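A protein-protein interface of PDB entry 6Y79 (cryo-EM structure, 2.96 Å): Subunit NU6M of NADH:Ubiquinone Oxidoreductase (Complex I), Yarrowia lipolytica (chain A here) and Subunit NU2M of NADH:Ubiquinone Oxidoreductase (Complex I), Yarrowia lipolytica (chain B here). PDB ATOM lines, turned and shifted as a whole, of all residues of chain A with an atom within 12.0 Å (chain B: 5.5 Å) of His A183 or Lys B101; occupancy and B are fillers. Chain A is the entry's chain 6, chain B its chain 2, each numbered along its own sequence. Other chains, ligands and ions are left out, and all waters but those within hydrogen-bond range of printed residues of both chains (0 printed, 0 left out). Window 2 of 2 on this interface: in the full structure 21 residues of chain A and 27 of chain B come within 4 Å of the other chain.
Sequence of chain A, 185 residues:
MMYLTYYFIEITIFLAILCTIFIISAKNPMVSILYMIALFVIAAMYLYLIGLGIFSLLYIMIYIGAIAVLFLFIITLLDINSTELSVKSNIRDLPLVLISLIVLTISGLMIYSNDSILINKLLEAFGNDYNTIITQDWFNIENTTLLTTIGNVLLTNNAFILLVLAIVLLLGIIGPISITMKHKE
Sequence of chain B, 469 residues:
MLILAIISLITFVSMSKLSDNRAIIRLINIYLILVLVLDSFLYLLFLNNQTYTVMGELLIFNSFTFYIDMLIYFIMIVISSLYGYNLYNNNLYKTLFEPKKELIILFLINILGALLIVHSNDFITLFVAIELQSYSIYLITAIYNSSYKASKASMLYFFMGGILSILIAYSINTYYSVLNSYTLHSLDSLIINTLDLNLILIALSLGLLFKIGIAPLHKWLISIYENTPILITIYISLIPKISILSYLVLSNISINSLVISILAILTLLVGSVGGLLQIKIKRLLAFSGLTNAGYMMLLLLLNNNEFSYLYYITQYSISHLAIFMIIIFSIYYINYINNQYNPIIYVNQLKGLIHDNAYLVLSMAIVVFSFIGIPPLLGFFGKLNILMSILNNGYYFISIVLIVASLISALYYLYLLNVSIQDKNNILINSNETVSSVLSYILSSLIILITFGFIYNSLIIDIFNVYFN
OE2 of Glu B102 is in hydrogen-bond range of NE2 of His A183 (2.8 Å).
The backbone carbonyl oxygen (O) of Val B13 lies within hydrogen-bond range of the side-chain amino group (NZ) of Lys B101. The backbone carbonyl oxygen (O) of Ser B16 is in hydrogen-bond range of the side-chain amino group (NZ) of Lys B101 (2.9 Å). O of Leu B18 sits at hydrogen-bond distance from ND2 of Asn B21, at 3.3 Å. The side-chain hydroxyl (OG) of Ser A178 sits close to the backbone carbonyl oxygen (O) of Ile A174, 3.3 Å away. The backbone carbonyl oxygen of Gly A175 lies within hydrogen-bond range of the side-chain hydroxyl of Ser A178 (2.6 Å). ND1 of His A183 lies close to SD of Met A181.
CG2 of Ile A174 touches CG2 of Ile B105 (3.96 Å). CB of Ser A178 touches CD of Glu B102, 3.6 Å away. His A183 touches Leu B18. CE1 of His A183 touches CD of Lys B101, 3.5 Å away. Lys A184 touches Leu B18 (NZ to CB, 3.4 Å).
His A183 touches just these residues of chain B: Leu B18, Lys B101 and Glu B102. Lys B101 touches one residue of chain A. No residue of chain A comes within 4 Å of Val B13. No residue of chain A comes within 4 Å of Ser B16. Of chain A, only His A183 (3.6 Å) and Lys A184 (3.4 Å) come within 4 Å of Leu B18. No residue of chain A comes within 4 Å of Lys B100. Printed residues of chain A within 4 Å of Glu B102: Ser A178 (3.6 Å) and His A183 (2.8 Å). Of the printed residues of chain B, Lys A184 touches Leu B18. Of the printed residues of chain B, Ser A178 touches Glu B102. Thr A180 touches none of the printed residues of chain B. Ile A179 touches none of the printed residues of chain B. The nearest printed residue of chain B that does not touch His A183 is Lys B100 (6.8 Å). The nearest residue of chain A that does not touch Lys B101 is Ser A178 (6.7 Å). The nearest printed residue of chain B that does not touch Lys A184 is Lys B17 (5.2 Å).
Hydrophobic or aromatic side chains of chain A within 4 Å of the printed part of chain B: Ile A174 and His A183. Of the 14 printed residues of chain B, 4 touch a printed residue of chain A. Among the printed residues, no Asp or Glu carboxylate lies within 4 Å of a Lys or Arg side-chain nitrogen of the other chain.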
ATOM      1  N   ILE A 173      -3.850  31.463  17.612  1.00  0.00           N
ATOM      2  CA  ILE A 173      -3.888  32.338  16.444  1.00  0.00           C
ATOM      3  C   ILE A 173      -4.953  31.878  15.452  1.00  0.00           C
ATOM      4  O   ILE A 173      -5.804  32.671  15.041  1.00  0.00           O
ATOM      5  CB  ILE A 173      -2.507  32.423  15.770  1.00  0.00           C
ATOM      6  CG1 ILE A 173      -1.504  33.130  16.671  1.00  0.00           C
ATOM      7  CG2 ILE A 173      -2.600  33.173  14.467  1.00  0.00           C
ATOM      8  CD1 ILE A 173      -0.083  32.984  16.209  1.00  0.00           C
ATOM      9  N   ILE A 174      -4.919  30.594  15.066  1.00  0.00           N
ATOM     10  CA  ILE A 174      -5.717  30.093  13.940  1.00  0.00           C
ATOM     11  C   ILE A 174      -7.207  30.157  14.256  1.00  0.00           C
ATOM     12  O   ILE A 174      -8.008  30.606  13.432  1.00  0.00           O
ATOM     13  CB  ILE A 174      -5.311  28.652  13.565  1.00  0.00           C
ATOM     14  CG1 ILE A 174      -3.834  28.517  13.203  1.00  0.00           C
ATOM     15  CG2 ILE A 174      -6.142  28.136  12.405  1.00  0.00           C
ATOM     16  CD1 ILE A 174      -3.400  29.253  12.030  1.00  0.00           C
ATOM     17  N   GLY A 175      -7.596  29.727  15.456  1.00  0.00           N
ATOM     18  CA  GLY A 175      -8.985  29.599  15.836  1.00  0.00           C
ATOM     19  C   GLY A 175      -9.854  30.845  15.819  1.00  0.00           C
ATOM     20  O   GLY A 175     -10.920  30.856  15.191  1.00  0.00           O
ATOM     21  N   PRO A 176      -9.450  31.898  16.545  1.00  0.00           N
ATOM     22  CA  PRO A 176     -10.186  33.171  16.467  1.00  0.00           C
ATOM     23  C   PRO A 176     -10.251  33.779  15.081  1.00  0.00           C
ATOM     24  O   PRO A 176     -11.235  34.448  14.755  1.00  0.00           O
ATOM     25  CB  PRO A 176      -9.400  34.064  17.427  1.00  0.00           C
ATOM     26  CG  PRO A 176      -8.884  33.139  18.430  1.00  0.00           C
ATOM     27  CD  PRO A 176      -8.543  31.887  17.703  1.00  0.00           C
ATOM     28  N   ILE A 177      -9.217  33.583  14.267  1.00  0.00           N
ATOM     29  CA  ILE A 177      -9.262  34.004  12.869  1.00  0.00           C
ATOM     30  C   ILE A 177     -10.293  33.185  12.111  1.00  0.00           C
ATOM     31  O   ILE A 177     -11.148  33.727  11.401  1.00  0.00           O
ATOM     32  CB  ILE A 177      -7.880  33.861  12.218  1.00  0.00           C
ATOM     33  CG1 ILE A 177      -6.895  34.867  12.788  1.00  0.00           C
ATOM     34  CG2 ILE A 177      -7.980  34.019  10.723  1.00  0.00           C
ATOM     35  CD1 ILE A 177      -5.502  34.605  12.318  1.00  0.00           C
ATOM     36  N   SER A 178     -10.201  31.858  12.247  1.00  0.00           N
ATOM     37  CA  SER A 178     -11.046  30.923  11.513  1.00  0.00           C
ATOM     38  C   SER A 178     -12.516  31.121  11.809  1.00  0.00           C
ATOM     39  O   SER A 178     -13.360  30.893  10.939  1.00  0.00           O
ATOM     40  CB  SER A 178     -10.670  29.502  11.875  1.00  0.00           C
ATOM     41  OG  SER A 178     -11.038  29.225  13.206  1.00  0.00           O
ATOM     42  N   ILE A 179     -12.841  31.525  13.030  1.00  0.00           N
ATOM     43  CA  ILE A 179     -14.221  31.851  13.353  1.00  0.00           C
ATOM     44  C   ILE A 179     -14.668  33.113  12.616  1.00  0.00           C
ATOM     45  O   ILE A 179     -15.646  33.096  11.863  1.00  0.00           O
ATOM     46  CB  ILE A 179     -14.388  32.014  14.869  1.00  0.00           C
ATOM     47  CG1 ILE A 179     -14.288  30.674  15.585  1.00  0.00           C
ATOM     48  CG2 ILE A 179     -15.695  32.580  15.131  1.00  0.00           C
ATOM     49  CD1 ILE A 179     -14.407  30.813  17.076  1.00  0.00           C
ATOM     50  N   THR A 180     -13.949  34.225  12.813  1.00  0.00           N
ATOM     51  CA  THR A 180     -14.497  35.565  12.617  1.00  0.00           C
ATOM     52  C   THR A 180     -14.154  36.187  11.275  1.00  0.00           C
ATOM     53  O   THR A 180     -14.105  37.418  11.185  1.00  0.00           O
ATOM     54  CB  THR A 180     -14.010  36.501  13.724  1.00  0.00           C
ATOM     55  OG1 THR A 180     -12.580  36.578  13.664  1.00  0.00           O
ATOM     56  CG2 THR A 180     -14.428  36.023  15.080  1.00  0.00           C
ATOM     57  N   MET A 181     -13.888  35.411  10.233  1.00  0.00           N
ATOM     58  CA  MET A 181     -13.431  36.073   9.018  1.00  0.00           C
ATOM     59  C   MET A 181     -14.554  36.271   8.008  1.00  0.00           C
ATOM     60  O   MET A 181     -14.697  37.361   7.435  1.00  0.00           O
ATOM     61  CB  MET A 181     -12.269  35.310   8.390  1.00  0.00           C
ATOM     62  CG  MET A 181     -11.690  36.151   7.290  1.00  0.00           C
ATOM     63  SD  MET A 181     -10.088  35.830   6.581  1.00  0.00           S
ATOM     64  CE  MET A 181     -10.273  36.879   5.139  1.00  0.00           C
ATOM     65  N   LYS A 182     -15.369  35.232   7.818  1.00  0.00           N
ATOM     66  CA  LYS A 182     -16.292  35.086   6.694  1.00  0.00           C
ATOM     67  C   LYS A 182     -15.544  35.289   5.373  1.00  0.00           C
ATOM     68  O   LYS A 182     -15.607  36.343   4.737  1.00  0.00           O
ATOM     69  CB  LYS A 182     -17.495  36.027   6.775  1.00  0.00           C
ATOM     70  CG  LYS A 182     -18.361  35.826   7.993  1.00  0.00           C
ATOM     71  CD  LYS A 182     -19.173  34.555   7.910  1.00  0.00           C
ATOM     72  CE  LYS A 182     -20.068  34.412   9.123  1.00  0.00           C
ATOM     73  NZ  LYS A 182     -20.873  33.174   9.042  1.00  0.00           N
ATOM     74  N   HIS A 183     -14.741  34.278   5.044  1.00  0.00           N
ATOM     75  CA  HIS A 183     -13.989  34.194   3.791  1.00  0.00           C
ATOM     76  C   HIS A 183     -14.873  34.460   2.582  1.00  0.00           C
ATOM     77  O   HIS A 183     -15.793  33.688   2.294  1.00  0.00           O
ATOM     78  CB  HIS A 183     -13.376  32.804   3.675  1.00  0.00           C
ATOM     79  CG  HIS A 183     -12.365  32.488   4.726  1.00  0.00           C
ATOM     80  ND1 HIS A 183     -11.066  32.948   4.679  1.00  0.00           N
ATOM     81  CD2 HIS A 183     -12.457  31.732   5.843  1.00  0.00           C
ATOM     82  CE1 HIS A 183     -10.406  32.500   5.731  1.00  0.00           C
ATOM     83  NE2 HIS A 183     -11.227  31.760   6.454  1.00  0.00           N
ATOM     84  N   LYS A 184     -14.534  35.536   1.869  1.00  0.00           N
ATOM     85  CA  LYS A 184     -15.283  36.165   0.763  1.00  0.00           C
ATOM     86  C   LYS A 184     -16.816  36.051   0.784  1.00  0.00           C
ATOM     87  O   LYS A 184     -17.446  36.154   1.838  1.00  0.00           O
ATOM     88  CB  LYS A 184     -14.779  35.643  -0.587  1.00  0.00           C
ATOM     89  CG  LYS A 184     -15.073  34.205  -0.922  1.00  0.00           C
ATOM     90  CD  LYS A 184     -14.666  33.990  -2.365  1.00  0.00           C
ATOM     91  CE  LYS A 184     -14.983  32.613  -2.846  1.00  0.00           C
ATOM     92  NZ  LYS A 184     -14.132  31.613  -2.124  1.00  0.00           N
ATOM     93  N   VAL B  13      -3.141  25.855   3.222  1.00  0.00           N
ATOM     94  CA  VAL B  13      -4.550  26.220   3.262  1.00  0.00           C
ATOM     95  C   VAL B  13      -4.713  27.734   3.250  1.00  0.00           C
ATOM     96  O   VAL B  13      -5.695  28.251   2.700  1.00  0.00           O
ATOM     97  CB  VAL B  13      -5.205  25.524   4.479  1.00  0.00           C
ATOM     98  CG1 VAL B  13      -6.477  26.193   4.959  1.00  0.00           C
ATOM     99  CG2 VAL B  13      -5.519  24.089   4.131  1.00  0.00           C
ATOM    100  N   SER B  14      -3.723  28.476   3.764  1.00  0.00           N
ATOM    101  CA  SER B  14      -3.765  29.936   3.667  1.00  0.00           C
ATOM    102  C   SER B  14      -3.679  30.434   2.228  1.00  0.00           C
ATOM    103  O   SER B  14      -4.148  31.535   1.926  1.00  0.00           O
ATOM    104  CB  SER B  14      -2.630  30.540   4.473  1.00  0.00           C
ATOM    105  OG  SER B  14      -1.375  30.129   3.974  1.00  0.00           O
ATOM    106  N   MET B  15      -3.102  29.640   1.333  1.00  0.00           N
ATOM    107  CA  MET B  15      -2.923  30.029  -0.054  1.00  0.00           C
ATOM    108  C   MET B  15      -3.946  29.433  -0.996  1.00  0.00           C
ATOM    109  O   MET B  15      -4.059  29.900  -2.134  1.00  0.00           O
ATOM    110  CB  MET B  15      -1.540  29.618  -0.520  1.00  0.00           C
ATOM    111  CG  MET B  15      -0.531  30.452   0.137  1.00  0.00           C
ATOM    112  SD  MET B  15       1.133  30.040  -0.297  1.00  0.00           S
ATOM    113  CE  MET B  15       1.910  31.401   0.563  1.00  0.00           C
ATOM    114  N   SER B  16      -4.661  28.407  -0.568  1.00  0.00           N
ATOM    115  CA  SER B  16      -5.729  27.876  -1.384  1.00  0.00           C
ATOM    116  C   SER B  16      -6.929  28.807  -1.335  1.00  0.00           C
ATOM    117  O   SER B  16      -7.076  29.627  -0.427  1.00  0.00           O
ATOM    118  CB  SER B  16      -6.128  26.490  -0.904  1.00  0.00           C
ATOM    119  OG  SER B  16      -5.002  25.642  -0.813  1.00  0.00           O
ATOM    120  N   LYS B  17      -7.786  28.682  -2.338  1.00  0.00           N
ATOM    121  CA  LYS B  17      -9.078  29.331  -2.290  1.00  0.00           C
ATOM    122  C   LYS B  17     -10.072  28.383  -1.636  1.00  0.00           C
ATOM    123  O   LYS B  17      -9.746  27.250  -1.274  1.00  0.00           O
ATOM    124  CB  LYS B  17      -9.526  29.740  -3.684  1.00  0.00           C
ATOM    125  CG  LYS B  17      -8.682  30.823  -4.324  1.00  0.00           C
ATOM    126  CD  LYS B  17      -9.243  31.211  -5.672  1.00  0.00           C
ATOM    127  CE  LYS B  17      -9.059  30.087  -6.682  1.00  0.00           C
ATOM    128  NZ  LYS B  17      -7.631  29.850  -7.033  1.00  0.00           N
ATOM    129  N   LEU B  18     -11.305  28.853  -1.474  1.00  0.00           N
ATOM    130  CA  LEU B  18     -12.309  28.039  -0.805  1.00  0.00           C
ATOM    131  C   LEU B  18     -12.868  26.987  -1.753  1.00  0.00           C
ATOM    132  O   LEU B  18     -13.548  26.054  -1.321  1.00  0.00           O
ATOM    133  CB  LEU B  18     -13.415  28.927  -0.246  1.00  0.00           C
ATOM    134  CG  LEU B  18     -13.278  29.753   1.041  1.00  0.00           C
ATOM    135  CD1 LEU B  18     -12.323  30.913   0.824  1.00  0.00           C
ATOM    136  CD2 LEU B  18     -14.657  30.280   1.327  1.00  0.00           C
ATOM    137  N   ASN B  21     -10.882  23.472  -0.827  1.00  0.00           N
ATOM    138  CA  ASN B  21     -10.908  22.903   0.525  1.00  0.00           C
ATOM    139  C   ASN B  21     -11.136  21.405   0.512  1.00  0.00           C
ATOM    140  O   ASN B  21     -10.347  20.652   1.096  1.00  0.00           O
ATOM    141  CB  ASN B  21     -12.011  23.549   1.361  1.00  0.00           C
ATOM    142  CG  ASN B  21     -11.716  24.975   1.720  1.00  0.00           C
ATOM    143  OD1 ASN B  21     -10.561  25.362   1.894  1.00  0.00           O
ATOM    144  ND2 ASN B  21     -12.765  25.767   1.863  1.00  0.00           N
ATOM    145  N   PRO B  99     -17.342  21.498   3.859  1.00  0.00           N
ATOM    146  CA  PRO B  99     -16.294  21.783   4.837  1.00  0.00           C
ATOM    147  C   PRO B  99     -15.907  23.251   4.842  1.00  0.00           C
ATOM    148  O   PRO B  99     -15.919  23.932   3.815  1.00  0.00           O
ATOM    149  CB  PRO B  99     -15.131  20.913   4.358  1.00  0.00           C
ATOM    150  CG  PRO B  99     -15.326  20.817   2.909  1.00  0.00           C
ATOM    151  CD  PRO B  99     -16.804  20.823   2.669  1.00  0.00           C
ATOM    152  N   LYS B 100     -15.560  23.736   6.029  1.00  0.00           N
ATOM    153  CA  LYS B 100     -14.989  25.064   6.140  1.00  0.00           C
ATOM    154  C   LYS B 100     -13.527  25.038   5.718  1.00  0.00           C
ATOM    155  O   LYS B 100     -12.948  23.989   5.432  1.00  0.00           O
ATOM    156  CB  LYS B 100     -15.113  25.598   7.559  1.00  0.00           C
ATOM    157  CG  LYS B 100     -16.506  25.934   7.987  1.00  0.00           C
ATOM    158  CD  LYS B 100     -17.251  26.782   6.991  1.00  0.00           C
ATOM    159  CE  LYS B 100     -18.637  27.076   7.508  1.00  0.00           C
ATOM    160  NZ  LYS B 100     -18.565  27.915   8.727  1.00  0.00           N
ATOM    161  N   LYS B 101     -12.914  26.218   5.707  1.00  0.00           N
ATOM    162  CA  LYS B 101     -11.540  26.337   5.242  1.00  0.00           C
ATOM    163  C   LYS B 101     -10.561  25.786   6.266  1.00  0.00           C
ATOM    164  O   LYS B 101      -9.562  25.154   5.906  1.00  0.00           O
ATOM    165  CB  LYS B 101     -11.238  27.801   4.929  1.00  0.00           C
ATOM    166  CG  LYS B 101      -9.884  28.068   4.329  1.00  0.00           C
ATOM    167  CD  LYS B 101      -9.777  29.526   3.972  1.00  0.00           C
ATOM    168  CE  LYS B 101      -8.383  29.911   3.546  1.00  0.00           C
ATOM    169  NZ  LYS B 101      -7.968  29.187   2.320  1.00  0.00           N
ATOM    170  N   GLU B 102     -10.847  25.991   7.548  1.00  0.00           N
ATOM    171  CA  GLU B 102      -9.945  25.656   8.641  1.00  0.00           C
ATOM    172  C   GLU B 102     -10.403  24.443   9.428  1.00  0.00           C
ATOM    173  O   GLU B 102     -10.078  24.309  10.606  1.00  0.00           O
ATOM    174  CB  GLU B 102      -9.815  26.834   9.588  1.00  0.00           C
ATOM    175  CG  GLU B 102      -9.115  27.981   8.991  1.00  0.00           C
ATOM    176  CD  GLU B 102     -10.041  29.013   8.372  1.00  0.00           C
ATOM    177  OE1 GLU B 102     -11.235  28.709   8.174  1.00  0.00           O
ATOM    178  OE2 GLU B 102      -9.567  30.129   8.066  1.00  0.00           O
ATOM    179  N   LEU B 103     -11.162  23.564   8.800  1.00  0.00           N
ATOM    180  CA  LEU B 103     -11.716  22.428   9.515  1.00  0.00           C
ATOM    181  C   LEU B 103     -10.668  21.346   9.723  1.00  0.00           C
ATOM    182  O   LEU B 103     -10.542  20.795  10.821  1.00  0.00           O
ATOM    183  CB  LEU B 103     -12.911  21.895   8.741  1.00  0.00           C
ATOM    184  CG  LEU B 103     -13.860  20.897   9.376  1.00  0.00           C
ATOM    185  CD1 LEU B 103     -14.378  21.410  10.682  1.00  0.00           C
ATOM    186  CD2 LEU B 103     -14.972  20.755   8.408  1.00  0.00           C
ATOM    187  N   ILE B 104      -9.893  21.047   8.681  1.00  0.00           N
ATOM    188  CA  ILE B 104      -8.901  19.988   8.753  1.00  0.00           C
ATOM    189  C   ILE B 104      -7.699  20.402   9.601  1.00  0.00           C
ATOM    190  O   ILE B 104      -7.040  19.537  10.200  1.00  0.00           O
ATOM    191  CB  ILE B 104      -8.548  19.571   7.309  1.00  0.00           C
ATOM    192  CG1 ILE B 104      -7.719  18.287   7.265  1.00  0.00           C
ATOM    193  CG2 ILE B 104      -7.933  20.718   6.538  1.00  0.00           C
ATOM    194  CD1 ILE B 104      -8.497  17.058   7.649  1.00  0.00           C
ATOM    195  N   ILE B 105      -7.448  21.713   9.717  1.00  0.00           N
ATOM    196  CA  ILE B 105      -6.476  22.248  10.670  1.00  0.00           C
ATOM    197  C   ILE B 105      -6.843  21.836  12.086  1.00  0.00           C
ATOM    198  O   ILE B 105      -6.032  21.263  12.823  1.00  0.00           O
ATOM    199  CB  ILE B 105      -6.406  23.781  10.570  1.00  0.00           C
ATOM    200  CG1 ILE B 105      -6.039  24.256   9.169  1.00  0.00           C
ATOM    201  CG2 ILE B 105      -5.441  24.326  11.594  1.00  0.00           C
ATOM    202  CD1 ILE B 105      -5.958  25.753   9.020  1.00  0.00           C
